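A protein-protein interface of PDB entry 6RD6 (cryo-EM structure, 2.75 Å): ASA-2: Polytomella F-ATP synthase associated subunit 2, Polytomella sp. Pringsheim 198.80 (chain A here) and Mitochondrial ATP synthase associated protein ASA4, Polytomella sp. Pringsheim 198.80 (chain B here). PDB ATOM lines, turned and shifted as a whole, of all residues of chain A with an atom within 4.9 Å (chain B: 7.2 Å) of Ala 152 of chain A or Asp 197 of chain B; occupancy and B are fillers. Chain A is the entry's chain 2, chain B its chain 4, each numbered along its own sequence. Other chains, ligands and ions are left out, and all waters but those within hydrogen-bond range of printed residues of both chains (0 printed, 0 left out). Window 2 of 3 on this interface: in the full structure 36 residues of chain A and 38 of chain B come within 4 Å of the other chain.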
ATOM      1  N   VAL A 125     -10.013   5.323  11.044  1.00  0.00           N
ATOM      2  CA  VAL A 125      -9.778   5.056   9.623  1.00  0.00           C
ATOM      3  C   VAL A 125      -9.902   6.334   8.799  1.00  0.00           C
ATOM      4  O   VAL A 125      -9.519   6.363   7.624  1.00  0.00           O
ATOM      5  CB  VAL A 125     -10.714   3.954   9.093  1.00  0.00           C
ATOM      6  CG1 VAL A 125     -10.708   2.749  10.013  1.00  0.00           C
ATOM      7  CG2 VAL A 125     -12.119   4.488   8.859  1.00  0.00           C
ATOM      8  N   ASN A 149     -17.922  -6.238  14.600  1.00  0.00           N
ATOM      9  CA  ASN A 149     -17.096  -6.900  13.592  1.00  0.00           C
ATOM     10  C   ASN A 149     -16.778  -5.883  12.502  1.00  0.00           C
ATOM     11  O   ASN A 149     -17.305  -5.921  11.389  1.00  0.00           O
ATOM     12  CB  ASN A 149     -17.796  -8.132  13.037  1.00  0.00           C
ATOM     13  CG  ASN A 149     -16.822  -9.150  12.482  1.00  0.00           C
ATOM     14  OD1 ASN A 149     -16.370  -9.037  11.346  1.00  0.00           O
ATOM     15  ND2 ASN A 149     -16.492 -10.151  13.287  1.00  0.00           N
ATOM     16  N   ASP A 150     -15.900  -4.945  12.846  1.00  0.00           N
ATOM     17  CA  ASP A 150     -15.499  -3.880  11.934  1.00  0.00           C
ATOM     18  C   ASP A 150     -14.317  -4.375  11.115  1.00  0.00           C
ATOM     19  O   ASP A 150     -13.201  -4.491  11.631  1.00  0.00           O
ATOM     20  CB  ASP A 150     -15.141  -2.612  12.705  1.00  0.00           C
ATOM     21  CG  ASP A 150     -15.476  -1.350  11.937  1.00  0.00           C
ATOM     22  OD1 ASP A 150     -16.637  -1.208  11.503  1.00  0.00           O
ATOM     23  OD2 ASP A 150     -14.583  -0.496  11.774  1.00  0.00           O
ATOM     24  N   VAL A 151     -14.560  -4.680   9.842  1.00  0.00           N
ATOM     25  CA  VAL A 151     -13.486  -5.183   8.999  1.00  0.00           C
ATOM     26  C   VAL A 151     -12.795  -4.055   8.244  1.00  0.00           C
ATOM     27  O   VAL A 151     -11.702  -4.256   7.710  1.00  0.00           O
ATOM     28  CB  VAL A 151     -14.000  -6.261   8.029  1.00  0.00           C
ATOM     29  CG1 VAL A 151     -14.696  -7.374   8.799  1.00  0.00           C
ATOM     30  CG2 VAL A 151     -14.904  -5.664   6.974  1.00  0.00           C
ATOM     31  N   ALA A 152     -13.406  -2.868   8.195  1.00  0.00           N
ATOM     32  CA  ALA A 152     -12.718  -1.705   7.641  1.00  0.00           C
ATOM     33  C   ALA A 152     -11.551  -1.297   8.526  1.00  0.00           C
ATOM     34  O   ALA A 152     -10.445  -1.032   8.035  1.00  0.00           O
ATOM     35  CB  ALA A 152     -13.698  -0.547   7.478  1.00  0.00           C
ATOM     36  N   LEU A 153     -11.775  -1.273   9.841  1.00  0.00           N
ATOM     37  CA  LEU A 153     -10.701  -0.986  10.781  1.00  0.00           C
ATOM     38  C   LEU A 153      -9.677  -2.111  10.809  1.00  0.00           C
ATOM     39  O   LEU A 153      -8.482  -1.858  10.978  1.00  0.00           O
ATOM     40  CB  LEU A 153     -11.282  -0.749  12.173  1.00  0.00           C
ATOM     41  CG  LEU A 153     -10.343  -0.367  13.314  1.00  0.00           C
ATOM     42  CD1 LEU A 153      -9.386   0.719  12.895  1.00  0.00           C
ATOM     43  CD2 LEU A 153     -11.160   0.095  14.481  1.00  0.00           C
ATOM     44  N   ALA A 154     -10.121  -3.354  10.614  1.00  0.00           N
ATOM     45  CA  ALA A 154      -9.184  -4.472  10.570  1.00  0.00           C
ATOM     46  C   ALA A 154      -8.306  -4.406   9.327  1.00  0.00           C
ATOM     47  O   ALA A 154      -7.108  -4.696   9.392  1.00  0.00           O
ATOM     48  CB  ALA A 154      -9.941  -5.796  10.628  1.00  0.00           C
ATOM     49  N   LYS A 155      -8.874  -3.971   8.200  1.00  0.00           N
ATOM     50  CA  LYS A 155      -8.090  -3.831   6.976  1.00  0.00           C
ATOM     51  C   LYS A 155      -7.113  -2.665   7.067  1.00  0.00           C
ATOM     52  O   LYS A 155      -5.956  -2.785   6.638  1.00  0.00           O
ATOM     53  CB  LYS A 155      -9.022  -3.661   5.779  1.00  0.00           C
ATOM     54  CG  LYS A 155      -9.607  -4.962   5.270  1.00  0.00           C
ATOM     55  CD  LYS A 155     -10.680  -4.710   4.234  1.00  0.00           C
ATOM     56  CE  LYS A 155     -11.324  -6.008   3.792  1.00  0.00           C
ATOM     57  NZ  LYS A 155     -10.392  -6.841   2.989  1.00  0.00           N
ATOM     58  N   ALA A 156      -7.553  -1.533   7.630  1.00  0.00           N
ATOM     59  CA  ALA A 156      -6.663  -0.386   7.804  1.00  0.00           C
ATOM     60  C   ALA A 156      -5.540  -0.700   8.788  1.00  0.00           C
ATOM     61  O   ALA A 156      -4.375  -0.336   8.562  1.00  0.00           O
ATOM     62  CB  ALA A 156      -7.462   0.829   8.267  1.00  0.00           C
ATOM     63  N   SER B 190     -24.158  -9.756   1.667  1.00  0.00           N
ATOM     64  CA  SER B 190     -23.548  -9.183   0.476  1.00  0.00           C
ATOM     65  C   SER B 190     -22.403 -10.072   0.017  1.00  0.00           C
ATOM     66  O   SER B 190     -21.949 -10.954   0.750  1.00  0.00           O
ATOM     67  CB  SER B 190     -23.035  -7.757   0.724  1.00  0.00           C
ATOM     68  OG  SER B 190     -24.101  -6.870   1.008  1.00  0.00           O
ATOM     69  N   ASN B 192     -19.171  -8.991  -1.247  1.00  0.00           N
ATOM     70  CA  ASN B 192     -17.937  -8.487  -0.663  1.00  0.00           C
ATOM     71  C   ASN B 192     -18.175  -8.161   0.803  1.00  0.00           C
ATOM     72  O   ASN B 192     -19.310  -7.897   1.213  1.00  0.00           O
ATOM     73  CB  ASN B 192     -17.440  -7.246  -1.405  1.00  0.00           C
ATOM     74  CG  ASN B 192     -18.529  -6.217  -1.607  1.00  0.00           C
ATOM     75  OD1 ASN B 192     -19.710  -6.554  -1.668  1.00  0.00           O
ATOM     76  ND2 ASN B 192     -18.137  -4.955  -1.716  1.00  0.00           N
ATOM     77  N   GLU B 193     -17.101  -8.187   1.595  1.00  0.00           N
ATOM     78  CA  GLU B 193     -17.250  -7.968   3.028  1.00  0.00           C
ATOM     79  C   GLU B 193     -17.225  -6.485   3.374  1.00  0.00           C
ATOM     80  O   GLU B 193     -17.624  -6.092   4.475  1.00  0.00           O
ATOM     81  CB  GLU B 193     -16.165  -8.727   3.791  1.00  0.00           C
ATOM     82  CG  GLU B 193     -14.759  -8.195   3.597  1.00  0.00           C
ATOM     83  CD  GLU B 193     -13.738  -8.971   4.404  1.00  0.00           C
ATOM     84  OE1 GLU B 193     -12.599  -9.145   3.923  1.00  0.00           O
ATOM     85  OE2 GLU B 193     -14.077  -9.414   5.520  1.00  0.00           O
ATOM     86  N   ASP B 194     -16.782  -5.639   2.441  1.00  0.00           N
ATOM     87  CA  ASP B 194     -16.761  -4.202   2.706  1.00  0.00           C
ATOM     88  C   ASP B 194     -18.161  -3.603   2.637  1.00  0.00           C
ATOM     89  O   ASP B 194     -18.553  -2.814   3.509  1.00  0.00           O
ATOM     90  CB  ASP B 194     -15.826  -3.498   1.725  1.00  0.00           C
ATOM     91  CG  ASP B 194     -14.371  -3.823   1.975  1.00  0.00           C
ATOM     92  OD1 ASP B 194     -14.018  -4.114   3.136  1.00  0.00           O
ATOM     93  OD2 ASP B 194     -13.576  -3.783   1.014  1.00  0.00           O
ATOM     94  N   ALA B 195     -18.931  -3.967   1.607  1.00  0.00           N
ATOM     95  CA  ALA B 195     -20.316  -3.516   1.518  1.00  0.00           C
ATOM     96  C   ALA B 195     -21.160  -4.127   2.627  1.00  0.00           C
ATOM     97  O   ALA B 195     -22.067  -3.472   3.157  1.00  0.00           O
ATOM     98  CB  ALA B 195     -20.897  -3.862   0.150  1.00  0.00           C
ATOM     99  N   ALA B 196     -20.849  -5.369   3.008  1.00  0.00           N
ATOM    100  CA  ALA B 196     -21.496  -5.987   4.159  1.00  0.00           C
ATOM    101  C   ALA B 196     -21.154  -5.252   5.448  1.00  0.00           C
ATOM    102  O   ALA B 196     -21.998  -5.137   6.339  1.00  0.00           O
ATOM    103  CB  ALA B 196     -21.096  -7.458   4.257  1.00  0.00           C
ATOM    104  N   ASP B 197     -19.935  -4.712   5.546  1.00  0.00           N
ATOM    105  CA  ASP B 197     -19.554  -3.933   6.719  1.00  0.00           C
ATOM    106  C   ASP B 197     -20.300  -2.605   6.769  1.00  0.00           C
ATOM    107  O   ASP B 197     -20.712  -2.163   7.848  1.00  0.00           O
ATOM    108  CB  ASP B 197     -18.040  -3.717   6.720  1.00  0.00           C
ATOM    109  CG  ASP B 197     -17.529  -3.035   7.985  1.00  0.00           C
ATOM    110  OD1 ASP B 197     -16.870  -3.719   8.793  1.00  0.00           O
ATOM    111  OD2 ASP B 197     -17.720  -1.813   8.156  1.00  0.00           O
ATOM    112  N   LYS B 198     -20.477  -1.955   5.612  1.00  0.00           N
ATOM    113  CA  LYS B 198     -21.256  -0.715   5.562  1.00  0.00           C
ATOM    114  C   LYS B 198     -22.708  -0.952   5.966  1.00  0.00           C
ATOM    115  O   LYS B 198     -23.278  -0.197   6.775  1.00  0.00           O
ATOM    116  CB  LYS B 198     -21.209  -0.112   4.159  1.00  0.00           C
ATOM    117  CG  LYS B 198     -19.827   0.184   3.621  1.00  0.00           C
ATOM    118  CD  LYS B 198     -19.122   1.269   4.401  1.00  0.00           C
ATOM    119  CE  LYS B 198     -17.834   1.668   3.703  1.00  0.00           C
ATOM    120  NZ  LYS B 198     -16.829   0.571   3.730  1.00  0.00           N
ATOM    121  N   VAL B 199     -23.309  -2.018   5.429  1.00  0.00           N
ATOM    122  CA  VAL B 199     -24.690  -2.361   5.753  1.00  0.00           C
ATOM    123  C   VAL B 199     -24.821  -2.765   7.218  1.00  0.00           C
ATOM    124  O   VAL B 199     -25.798  -2.404   7.885  1.00  0.00           O
ATOM    125  CB  VAL B 199     -25.182  -3.457   4.788  1.00  0.00           C
ATOM    126  CG1 VAL B 199     -26.523  -3.994   5.201  1.00  0.00           C
ATOM    127  CG2 VAL B 199     -25.287  -2.894   3.387  1.00  0.00           C
ATOM    128  N   SER B 200     -23.814  -3.450   7.766  1.00  0.00           N
ATOM    129  CA  SER B 200     -23.874  -3.859   9.165  1.00  0.00           C
ATOM    130  C   SER B 200     -23.718  -2.669  10.101  1.00  0.00           C
ATOM    131  O   SER B 200     -24.344  -2.630  11.163  1.00  0.00           O
ATOM    132  CB  SER B 200     -22.804  -4.905   9.461  1.00  0.00           C
ATOM    133  OG  SER B 200     -21.537  -4.300   9.597  1.00  0.00           O
ATOM    134  N   LYS B 201     -22.906  -1.680   9.719  1.00  0.00           N
ATOM    135  CA  LYS B 201     -22.772  -0.488  10.549  1.00  0.00           C
ATOM    136  C   LYS B 201     -24.059   0.331  10.554  1.00  0.00           C
ATOM    137  O   LYS B 201     -24.481   0.823  11.609  1.00  0.00           O
ATOM    138  CB  LYS B 201     -21.588   0.354  10.078  1.00  0.00           C
ATOM    139  CG  LYS B 201     -20.242  -0.230  10.479  1.00  0.00           C
ATOM    140  CD  LYS B 201     -19.089   0.670  10.088  1.00  0.00           C
ATOM    141  CE  LYS B 201     -18.941   1.820  11.062  1.00  0.00           C
ATOM    142  NZ  LYS B 201     -17.658   2.550  10.875  1.00  0.00           N
ATOM    143  N   GLU B 202     -24.725   0.438   9.398  1.00  0.00           N
ATOM    144  CA  GLU B 202     -26.018   1.127   9.368  1.00  0.00           C
ATOM    145  C   GLU B 202     -27.089   0.354  10.139  1.00  0.00           C
ATOM    146  O   GLU B 202     -27.917   0.953  10.846  1.00  0.00           O
ATOM    147  CB  GLU B 202     -26.456   1.359   7.924  1.00  0.00           C
ATOM    148  CG  GLU B 202     -25.530   2.252   7.126  1.00  0.00           C
ATOM    149  CD  GLU B 202     -25.716   2.088   5.631  1.00  0.00           C
ATOM    150  OE1 GLU B 202     -25.052   2.815   4.864  1.00  0.00           O
ATOM    151  OE2 GLU B 202     -26.526   1.231   5.221  1.00  0.00           O
ATOM    152  N   PHE B 203     -27.061  -0.982  10.046  1.00  0.00           N
ATOM    153  CA  PHE B 203     -28.017  -1.805  10.779  1.00  0.00           C
ATOM    154  C   PHE B 203     -27.807  -1.696  12.278  1.00  0.00           C
ATOM    155  O   PHE B 203     -28.775  -1.655  13.036  1.00  0.00           O
ATOM    156  CB  PHE B 203     -27.919  -3.271  10.358  1.00  0.00           C
ATOM    157  CG  PHE B 203     -28.799  -4.191  11.171  1.00  0.00           C
ATOM    158  CD1 PHE B 203     -30.156  -4.259  10.922  1.00  0.00           C
ATOM    159  CD2 PHE B 203     -28.271  -4.978  12.189  1.00  0.00           C
ATOM    160  CE1 PHE B 203     -30.968  -5.088  11.665  1.00  0.00           C
ATOM    161  CE2 PHE B 203     -29.086  -5.803  12.938  1.00  0.00           C
ATOM    162  CZ  PHE B 203     -30.431  -5.860  12.670  1.00  0.00           C
ATOM    163  N   PHE B 204     -26.556  -1.677  12.729  1.00  0.00           N
ATOM    164  CA  PHE B 204     -26.324  -1.632  14.163  1.00  0.00           C
ATOM    165  C   PHE B 204     -26.541  -0.234  14.713  1.00  0.00           C
ATOM    166  O   PHE B 204     -26.868  -0.093  15.894  1.00  0.00           O
ATOM    167  CB  PHE B 204     -24.935  -2.165  14.488  1.00  0.00           C
ATOM    168  CG  PHE B 204     -24.890  -3.658  14.592  1.00  0.00           C
ATOM    169  CD1 PHE B 204     -24.070  -4.401  13.769  1.00  0.00           C
ATOM    170  CD2 PHE B 204     -25.695  -4.318  15.501  1.00  0.00           C
ATOM    171  CE1 PHE B 204     -24.042  -5.773  13.857  1.00  0.00           C
ATOM    172  CE2 PHE B 204     -25.672  -5.691  15.594  1.00  0.00           C
ATOM    173  CZ  PHE B 204     -24.845  -6.418  14.771  1.00  0.00           C
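Asp 150 of chain A touches Asp 197 of chain B. Val 151 of chain A touches Glu 193 of chain B (CG2 to O, 3.7 Å). N of Ala 152 of chain A touches OD1 of Asp 197 of chain B (3.6 Å). Lys 155 of chain A touches Asp 194 of chain B.
OD2 of Asp 150 of chain A sits close to N of Leu 153 of chain A (3.5 Å). O of Asp 197 of chain B is in hydrogen-bond range of OG of Ser 200 of chain B (2.9 Å).
Of the 14 printed residues of chain B, 4 touch a printed residue of chain A. Hydrophobic or aromatic side chains of chain A within 4 Å of the printed part of chain B: Val 151. Among the printed residues, 8 pairs touch across the chains.
The side-chain amino group of Lys 201 of chain B lies within salt-bridge range of the side-chain carboxylate of Asp 150 of chain A. OD1 of Asp 197 of chain B is in hydrogen-bond range of N of Val 151 of chain A (2.7 Å). The side-chain amino group of Lys 155 of chain A is in salt-bridge range of the side-chain carboxylate of Glu 193 of chain B (3.3 Å). The side-chain carboxylate (OD1) of Asp 197 of chain B sits close to the backbone carbonyl oxygen (O) of Asn 149 of chain A, 3.4 Å away.
Of chain B, only Asp 197 comes within 4 Å of Ala 152 of chain A. Asp 197 of chain B touches just these residues of chain A: Asn 149 (3.4 Å), Asp 150 (3.4 Å), Val 151 (2.7 Å) and Ala 152 (3.6 Å). Of the printed residues of chain A, Glu 193 of chain B touches Val 151 (3.7 Å) and Lys 155 (3.3 Å). Printed residues of chain B within 4 Å of Lys 155 of chain A: Glu 193 and Asp 194. Of the printed residues of chain B, Asn 149 of chain A touches Asp 197 (3.4 Å). The nearest residue of chain B that does not touch Ala 152 of chain A is Lys 198 of chain B (5.0 Å). The nearest printed residue of chain A that does not touch Glu 193 of chain B is Asn 149 of chain A (6.3 Å).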
